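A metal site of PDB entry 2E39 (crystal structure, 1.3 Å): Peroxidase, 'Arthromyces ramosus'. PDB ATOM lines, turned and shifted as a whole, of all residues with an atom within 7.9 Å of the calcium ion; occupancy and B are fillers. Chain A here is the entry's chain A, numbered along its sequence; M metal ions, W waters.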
ATOM      1  N   ILE A  53       7.264  10.627  -8.382  1.00  0.00           N
ATOM      2  CA  ILE A  53       7.965  11.881  -8.467  1.00  0.00           C
ATOM      3  C   ILE A  53       7.137  13.038  -9.000  1.00  0.00           C
ATOM      4  O   ILE A  53       7.251  14.145  -8.475  1.00  0.00           O
ATOM      5  CB  ILE A  53       9.273  11.720  -9.286  1.00  0.00           C
ATOM      6  CG1 ILE A  53      10.226  10.794  -8.516  1.00  0.00           C
ATOM      7  CG2 ILE A  53       9.881  13.043  -9.679  1.00  0.00           C
ATOM      8  CD1 ILE A  53      11.402  10.241  -9.328  1.00  0.00           C
ATOM      9  N   VAL A  54       6.284  12.817  -9.978  1.00  0.00           N
ATOM     10  CA  VAL A  54       5.513  13.920 -10.543  1.00  0.00           C
ATOM     11  C   VAL A  54       4.521  14.433  -9.513  1.00  0.00           C
ATOM     12  O   VAL A  54       4.309  15.617  -9.319  1.00  0.00           O
ATOM     13  CB  VAL A  54       4.847  13.544 -11.885  1.00  0.00           C
ATOM     14  CG1 VAL A  54       3.745  12.499 -11.714  1.00  0.00           C
ATOM     15  CG2 VAL A  54       4.360  14.786 -12.595  1.00  0.00           C
ATOM     16  N   PHE A  55       3.916  13.519  -8.778  1.00  0.00           N
ATOM     17  CA  PHE A  55       3.022  13.826  -7.694  1.00  0.00           C
ATOM     18  C   PHE A  55       3.754  14.557  -6.588  1.00  0.00           C
ATOM     19  O   PHE A  55       3.327  15.614  -6.080  1.00  0.00           O
ATOM     20  CB  PHE A  55       2.335  12.554  -7.180  1.00  0.00           C
ATOM     21  CG  PHE A  55       1.422  12.675  -5.969  1.00  0.00           C
ATOM     22  CD1 PHE A  55       0.593  13.753  -5.742  1.00  0.00           C
ATOM     23  CD2 PHE A  55       1.406  11.647  -5.047  1.00  0.00           C
ATOM     24  CE1 PHE A  55      -0.216  13.852  -4.633  1.00  0.00           C
ATOM     25  CE2 PHE A  55       0.617  11.738  -3.920  1.00  0.00           C
ATOM     26  CZ  PHE A  55      -0.219  12.826  -3.715  1.00  0.00           C
ATOM     27  N   HIS A  56       4.903  14.034  -6.156  1.00  0.00           N
ATOM     28  CA  HIS A  56       5.578  14.641  -5.043  1.00  0.00           C
ATOM     29  C   HIS A  56       6.274  15.945  -5.420  1.00  0.00           C
ATOM     30  O   HIS A  56       6.553  16.775  -4.517  1.00  0.00           O
ATOM     31  CB  HIS A  56       6.574  13.679  -4.390  1.00  0.00           C
ATOM     32  CG  HIS A  56       5.966  12.430  -3.866  1.00  0.00           C
ATOM     33  ND1 HIS A  56       6.636  11.482  -3.154  1.00  0.00           N
ATOM     34  CD2 HIS A  56       4.675  12.005  -3.962  1.00  0.00           C
ATOM     35  CE1 HIS A  56       5.783  10.505  -2.833  1.00  0.00           C
ATOM     36  NE2 HIS A  56       4.610  10.802  -3.327  1.00  0.00           N
ATOM     37  N   ASP A  57       6.561  16.164  -6.700  1.00  0.00           N
ATOM     38  CA  ASP A  57       7.022  17.477  -7.132  1.00  0.00           C
ATOM     39  C   ASP A  57       5.856  18.470  -7.064  1.00  0.00           C
ATOM     40  O   ASP A  57       5.988  19.508  -6.413  1.00  0.00           O
ATOM     41  CB  ASP A  57       7.618  17.450  -8.533  1.00  0.00           C
ATOM     42  CG  ASP A  57       8.247  18.795  -8.863  1.00  0.00           C
ATOM     43  OD1 ASP A  57       8.760  19.436  -7.940  1.00  0.00           O
ATOM     44  OD2 ASP A  57       8.249  19.162 -10.059  1.00  0.00           O
ATOM     45  N   ALA A  58       4.727  18.151  -7.668  1.00  0.00           N
ATOM     46  CA  ALA A  58       3.653  19.103  -7.841  1.00  0.00           C
ATOM     47  C   ALA A  58       2.928  19.416  -6.545  1.00  0.00           C
ATOM     48  O   ALA A  58       2.495  20.558  -6.378  1.00  0.00           O
ATOM     49  CB  ALA A  58       2.678  18.577  -8.906  1.00  0.00           C
ATOM     50  N   ILE A  59       2.796  18.422  -5.689  1.00  0.00           N
ATOM     51  CA  ILE A  59       1.957  18.593  -4.515  1.00  0.00           C
ATOM     52  C   ILE A  59       2.648  19.460  -3.471  1.00  0.00           C
ATOM     53  O   ILE A  59       2.001  19.819  -2.494  1.00  0.00           O
ATOM     54  CB  ILE A  59       1.492  17.215  -3.954  1.00  0.00           C
ATOM     55  CG1 ILE A  59       0.098  17.309  -3.311  1.00  0.00           C
ATOM     56  CG2 ILE A  59       2.561  16.582  -3.073  1.00  0.00           C
ATOM     57  CD1 ILE A  59      -1.015  17.720  -4.250  1.00  0.00           C
ATOM     58  N   GLY A  60       3.921  19.818  -3.660  1.00  0.00           N
ATOM     59  CA  GLY A  60       4.576  20.782  -2.775  1.00  0.00           C
ATOM     60  C   GLY A  60       4.144  22.220  -3.161  1.00  0.00           C
ATOM     61  O   GLY A  60       4.855  22.998  -3.775  1.00  0.00           O
ATOM     62  N   PHE A  61       2.886  22.484  -2.803  1.00  0.00           N
ATOM     63  CA  PHE A  61       2.129  23.676  -3.203  1.00  0.00           C
ATOM     64  C   PHE A  61       1.018  23.795  -2.146  1.00  0.00           C
ATOM     65  O   PHE A  61       0.232  22.888  -1.990  1.00  0.00           O
ATOM     66  CB  PHE A  61       1.608  23.547  -4.608  1.00  0.00           C
ATOM     67  CG  PHE A  61       0.851  24.761  -5.085  1.00  0.00           C
ATOM     68  CD1 PHE A  61       1.555  25.877  -5.465  1.00  0.00           C
ATOM     69  CD2 PHE A  61      -0.521  24.810  -5.179  1.00  0.00           C
ATOM     70  CE1 PHE A  61       0.937  27.037  -5.888  1.00  0.00           C
ATOM     71  CE2 PHE A  61      -1.169  25.979  -5.566  1.00  0.00           C
ATOM     72  CZ  PHE A  61      -0.433  27.071  -5.949  1.00  0.00           C
ATOM     73  N   GLY A  73       5.527  26.640  -1.358  1.00  0.00           N
ATOM     74  CA  GLY A  73       6.015  25.776  -2.412  1.00  0.00           C
ATOM     75  C   GLY A  73       5.664  26.222  -3.810  1.00  0.00           C
ATOM     76  O   GLY A  73       4.640  26.891  -3.987  1.00  0.00           O
ATOM     77  N   GLY A  74       6.486  25.863  -4.793  1.00  0.00           N
ATOM     78  CA  GLY A  74       6.262  26.308  -6.155  1.00  0.00           C
ATOM     79  C   GLY A  74       5.626  25.271  -7.061  1.00  0.00           C
ATOM     80  O   GLY A  74       5.598  25.499  -8.274  1.00  0.00           O
ATOM     81  N   GLY A  75       5.088  24.179  -6.502  1.00  0.00           N
ATOM     82  CA  GLY A  75       4.337  23.234  -7.350  1.00  0.00           C
ATOM     83  C   GLY A  75       5.264  22.441  -8.254  1.00  0.00           C
ATOM     84  O   GLY A  75       6.280  21.892  -7.840  1.00  0.00           O
ATOM     85  N   ALA A  76       4.911  22.342  -9.525  1.00  0.00           N
ATOM     86  CA  ALA A  76       5.537  21.508 -10.533  1.00  0.00           C
ATOM     87  C   ALA A  76       6.829  22.149 -11.037  1.00  0.00           C
ATOM     88  O   ALA A  76       7.024  22.307 -12.243  1.00  0.00           O
ATOM     89  CB  ALA A  76       4.517  21.225 -11.628  1.00  0.00           C
ATOM     90  N   ASP A  77       7.696  22.528 -10.127  1.00  0.00           N
ATOM     91  CA  ASP A  77       8.855  23.385 -10.344  1.00  0.00           C
ATOM     92  C   ASP A  77      10.170  22.624 -10.400  1.00  0.00           C
ATOM     93  O   ASP A  77      11.245  23.242 -10.485  1.00  0.00           O
ATOM     94  CB  ASP A  77       8.903  24.442  -9.250  1.00  0.00           C
ATOM     95  CG  ASP A  77       8.984  23.902  -7.836  1.00  0.00           C
ATOM     96  OD1 ASP A  77       9.015  22.662  -7.633  1.00  0.00           O
ATOM     97  OD2 ASP A  77       9.018  24.738  -6.912  1.00  0.00           O
ATOM     98  N   GLY A  78      10.128  21.297 -10.329  1.00  0.00           N
ATOM     99  CA  GLY A  78      11.351  20.510 -10.359  1.00  0.00           C
ATOM    100  C   GLY A  78      12.133  20.593  -9.054  1.00  0.00           C
ATOM    101  O   GLY A  78      13.279  20.129  -8.989  1.00  0.00           O
ATOM    102  N   SER A  79      11.575  21.182  -8.010  1.00  0.00           N
ATOM    103  CA  SER A  79      12.254  21.281  -6.727  1.00  0.00           C
ATOM    104  C   SER A  79      12.701  19.962  -6.129  1.00  0.00           C
ATOM    105  O   SER A  79      13.748  19.917  -5.482  1.00  0.00           O
ATOM    106  CB  SER A  79      11.351  22.014  -5.732  1.00  0.00           C
ATOM    107  OG  SER A  79      10.232  21.211  -5.325  1.00  0.00           O
ATOM    108  N   ILE A  80      11.972  18.881  -6.398  1.00  0.00           N
ATOM    109  CA  ILE A  80      12.321  17.557  -5.902  1.00  0.00           C
ATOM    110  C   ILE A  80      13.655  17.114  -6.490  1.00  0.00           C
ATOM    111  O   ILE A  80      14.368  16.311  -5.860  1.00  0.00           O
ATOM    112  CB  ILE A  80      11.182  16.546  -6.127  1.00  0.00           C
ATOM    113  CG1 ILE A  80      11.353  15.318  -5.236  1.00  0.00           C
ATOM    114  CG2 ILE A  80      11.008  16.252  -7.606  1.00  0.00           C
ATOM    115  CD1 ILE A  80      10.187  14.356  -5.277  1.00  0.00           C
ATOM    116  N   ILE A  81      14.039  17.620  -7.675  1.00  0.00           N
ATOM    117  CA  ILE A  81      15.370  17.369  -8.239  1.00  0.00           C
ATOM    118  C   ILE A  81      16.357  18.428  -7.802  1.00  0.00           C
ATOM    119  O   ILE A  81      17.436  18.121  -7.275  1.00  0.00           O
ATOM    120  CB  ILE A  81      15.343  17.259  -9.768  1.00  0.00           C
ATOM    121  CG1 ILE A  81      14.410  16.142 -10.257  1.00  0.00           C
ATOM    122  CG2 ILE A  81      16.730  17.048 -10.322  1.00  0.00           C
ATOM    123  CD1 ILE A  81      14.245  16.044 -11.747  1.00  0.00           C
ATOM    124  N   HIS A  83      16.451  20.521  -5.401  1.00  0.00           N
ATOM    125  CA  HIS A  83      16.602  20.505  -3.967  1.00  0.00           C
ATOM    126  C   HIS A  83      16.352  19.126  -3.369  1.00  0.00           C
ATOM    127  O   HIS A  83      15.792  18.943  -2.287  1.00  0.00           O
ATOM    128  CB  HIS A  83      15.654  21.506  -3.311  1.00  0.00           C
ATOM    129  CG  HIS A  83      15.901  22.894  -3.857  1.00  0.00           C
ATOM    130  ND1 HIS A  83      17.056  23.572  -3.555  1.00  0.00           N
ATOM    131  CD2 HIS A  83      15.198  23.709  -4.680  1.00  0.00           C
ATOM    132  CE1 HIS A  83      17.034  24.757  -4.167  1.00  0.00           C
ATOM    133  NE2 HIS A  83      15.924  24.871  -4.856  1.00  0.00           N
ATOM    134  N   GLU A  87      14.459  17.511  -0.100  1.00  0.00           N
ATOM    135  CA  GLU A  87      13.156  16.875  -0.264  1.00  0.00           C
ATOM    136  C   GLU A  87      13.260  15.373  -0.137  1.00  0.00           C
ATOM    137  O   GLU A  87      12.279  14.766   0.302  1.00  0.00           O
ATOM    138  CB  GLU A  87      12.530  17.270  -1.611  1.00  0.00           C
ATOM    139  CG  GLU A  87      12.183  18.759  -1.661  1.00  0.00           C
ATOM    140  CD  GLU A  87      11.271  19.172  -2.792  1.00  0.00           C
ATOM    141  OE1 GLU A  87      10.487  18.355  -3.293  1.00  0.00           O
ATOM    142  OE2 GLU A  87      11.297  20.367  -3.144  1.00  0.00           O
ATOM    143  N   GLY A 115      11.374  20.947 -13.929  1.00  0.00           N
ATOM    144  CA  GLY A 115       9.895  20.818 -13.774  1.00  0.00           C
ATOM    145  C   GLY A 115       9.303  20.337 -15.079  1.00  0.00           C
ATOM    146  O   GLY A 115       8.398  19.486 -15.075  1.00  0.00           O
ATOM    147  N   ILE A 118      10.150  16.477 -15.589  1.00  0.00           N
ATOM    148  CA  ILE A 118       9.348  15.516 -14.811  1.00  0.00           C
ATOM    149  C   ILE A 118       8.005  15.302 -15.484  1.00  0.00           C
ATOM    150  O   ILE A 118       7.527  14.178 -15.622  1.00  0.00           O
ATOM    151  CB  ILE A 118       9.233  15.942 -13.339  1.00  0.00           C
ATOM    152  CG1 ILE A 118      10.581  15.878 -12.640  1.00  0.00           C
ATOM    153  CG2 ILE A 118       8.166  15.163 -12.594  1.00  0.00           C
ATOM    154  CD1 ILE A 118      10.605  16.530 -11.256  1.00  0.00           C
ATOM    155  N   SER A 145      13.726  27.070  -8.642  1.00  0.00           N
ATOM    156  CA  SER A 145      12.859  26.630  -7.564  1.00  0.00           C
ATOM    157  C   SER A 145      13.470  26.864  -6.190  1.00  0.00           C
ATOM    158  O   SER A 145      14.692  26.913  -6.093  1.00  0.00           O
ATOM    159  CB  SER A 145      12.525  25.147  -7.688  1.00  0.00           C
ATOM    160  OG  SER A 145      13.692  24.377  -7.605  1.00  0.00           O
ATOM    161  N   GLN A 146      12.641  26.962  -5.191  1.00  0.00           N
ATOM    162  CA  GLN A 146      12.997  26.888  -3.790  1.00  0.00           C
ATOM    163  C   GLN A 146      12.590  25.507  -3.262  1.00  0.00           C
ATOM    164  O   GLN A 146      11.711  24.837  -3.867  1.00  0.00           O
ATOM    165  CB  GLN A 146      12.324  27.956  -2.937  1.00  0.00           C
ATOM    166  CG  GLN A 146      12.667  29.400  -3.213  1.00  0.00           C
ATOM    167  CD  GLN A 146      11.577  30.383  -2.815  1.00  0.00           C
ATOM    168  OE1 GLN A 146      10.971  31.031  -3.686  1.00  0.00           O
ATOM    169  NE2 GLN A 146      11.298  30.523  -1.528  1.00  0.00           N
ATOM    170  N   PRO A 147      13.158  25.038  -2.159  1.00  0.00           N
ATOM    171  CA  PRO A 147      12.743  23.715  -1.662  1.00  0.00           C
ATOM    172  C   PRO A 147      11.264  23.702  -1.301  1.00  0.00           C
ATOM    173  O   PRO A 147      10.733  24.665  -0.729  1.00  0.00           O
ATOM    174  CB  PRO A 147      13.592  23.509  -0.415  1.00  0.00           C
ATOM    175  CG  PRO A 147      14.786  24.415  -0.640  1.00  0.00           C
ATOM    176  CD  PRO A 147      14.222  25.635  -1.317  1.00  0.00           C
ATOM    177  N   SER A 148      10.569  22.620  -1.609  1.00  0.00           N
ATOM    178  CA  SER A 148       9.242  22.459  -1.032  1.00  0.00           C
ATOM    179  C   SER A 148       9.261  22.544   0.483  1.00  0.00           C
ATOM    180  O   SER A 148      10.148  21.974   1.109  1.00  0.00           O
ATOM    181  CB  SER A 148       8.704  21.044  -1.409  1.00  0.00           C
ATOM    182  OG  SER A 148       7.426  20.861  -0.795  1.00  0.00           O
ATOM    183  N   PRO A 149       8.270  23.159   1.094  1.00  0.00           N
ATOM    184  CA  PRO A 149       8.036  22.983   2.522  1.00  0.00           C
ATOM    185  C   PRO A 149       7.873  21.493   2.820  1.00  0.00           C
ATOM    186  O   PRO A 149       7.426  20.700   1.999  1.00  0.00           O
ATOM    187  CB  PRO A 149       6.764  23.767   2.793  1.00  0.00           C
ATOM    188  CG  PRO A 149       6.720  24.763   1.703  1.00  0.00           C
ATOM    189  CD  PRO A 149       7.303  24.070   0.498  1.00  0.00           C
ATOM    190  N   LEU A 283       0.331  23.221 -11.211  1.00  0.00           N
ATOM    191  CA  LEU A 283       0.347  23.851  -9.905  1.00  0.00           C
ATOM    192  C   LEU A 283       1.615  24.714  -9.823  1.00  0.00           C
ATOM    193  O   LEU A 283       2.688  24.194 -10.054  1.00  0.00           O
ATOM    194  CB  LEU A 283       0.298  22.813  -8.796  1.00  0.00           C
ATOM    195  CG  LEU A 283      -0.977  21.961  -8.690  1.00  0.00           C
ATOM    196  CD1 LEU A 283      -0.850  20.985  -7.518  1.00  0.00           C
ATOM    197  CD2 LEU A 283      -2.223  22.803  -8.489  1.00  0.00           C
ATOM    198  N   PHE A 285       1.948  27.472 -11.693  1.00  0.00           N
ATOM    199  CA  PHE A 285       2.128  28.020 -13.030  1.00  0.00           C
ATOM    200  C   PHE A 285       0.835  28.454 -13.704  1.00  0.00           C
ATOM    201  O   PHE A 285      -0.235  27.953 -13.363  1.00  0.00           O
ATOM    202  CB  PHE A 285       2.819  27.017 -13.985  1.00  0.00           C
ATOM    203  CG  PHE A 285       4.200  26.661 -13.450  1.00  0.00           C
ATOM    204  CD1 PHE A 285       4.323  25.588 -12.582  1.00  0.00           C
ATOM    205  CD2 PHE A 285       5.296  27.426 -13.760  1.00  0.00           C
ATOM    206  CE1 PHE A 285       5.541  25.309 -11.986  1.00  0.00           C
ATOM    207  CE2 PHE A 285       6.538  27.118 -13.226  1.00  0.00           C
ATOM    208  CZ  PHE A 285       6.632  26.041 -12.360  1.00  0.00           C
HETATM  209 CA    CA M   1       8.004  20.963  -6.329  1.00  0.00          CA
HETATM  210  O   HOH W   1       8.300  19.202  -4.611  1.00  0.00           O
HETATM  211  O   HOH W   2       7.341  22.281  -4.507  1.00  0.00           O
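Four residues have an atom within 4 Å of the calcium ion: Asp 57, Gly 75, Asp 77 and Ser 79.
Water W1 lies within hydrogen-bond range of OE1 of Glu 87 (2.7 Å) and O of His 56 (3.0 Å).
The side-chain carboxylate (OD2) of Asp 57 sits at hydrogen-bond distance from the backbone NH (N) of Gly 78 (2.9 Å). N of Gly 74 sits close to OD2 of Asp 77 (3.5 Å). OG of Ser 79 sits close to OE2 of Glu 87 (2.6 Å). The backbone carbonyl oxygen (O) of Gly 60 lies within hydrogen-bond range of the backbone NH (N) of Gly 75, 3.0 Å away.
The calcium ion is bound by water W2 (2.3 Å), the side-chain carboxylate (OD1) of Asp 57 (2.3 Å), the side-chain carboxylate (OD1) of Asp 77 (2.4 Å), the side-chain hydroxyl (OG) of Ser 79 (2.5 Å), the backbone carbonyl oxygen (O) of Gly 75 (2.5 Å), water W1 (2.5 Å) and the backbone carbonyl oxygen (O) of Asp 57 (2.5 Å).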
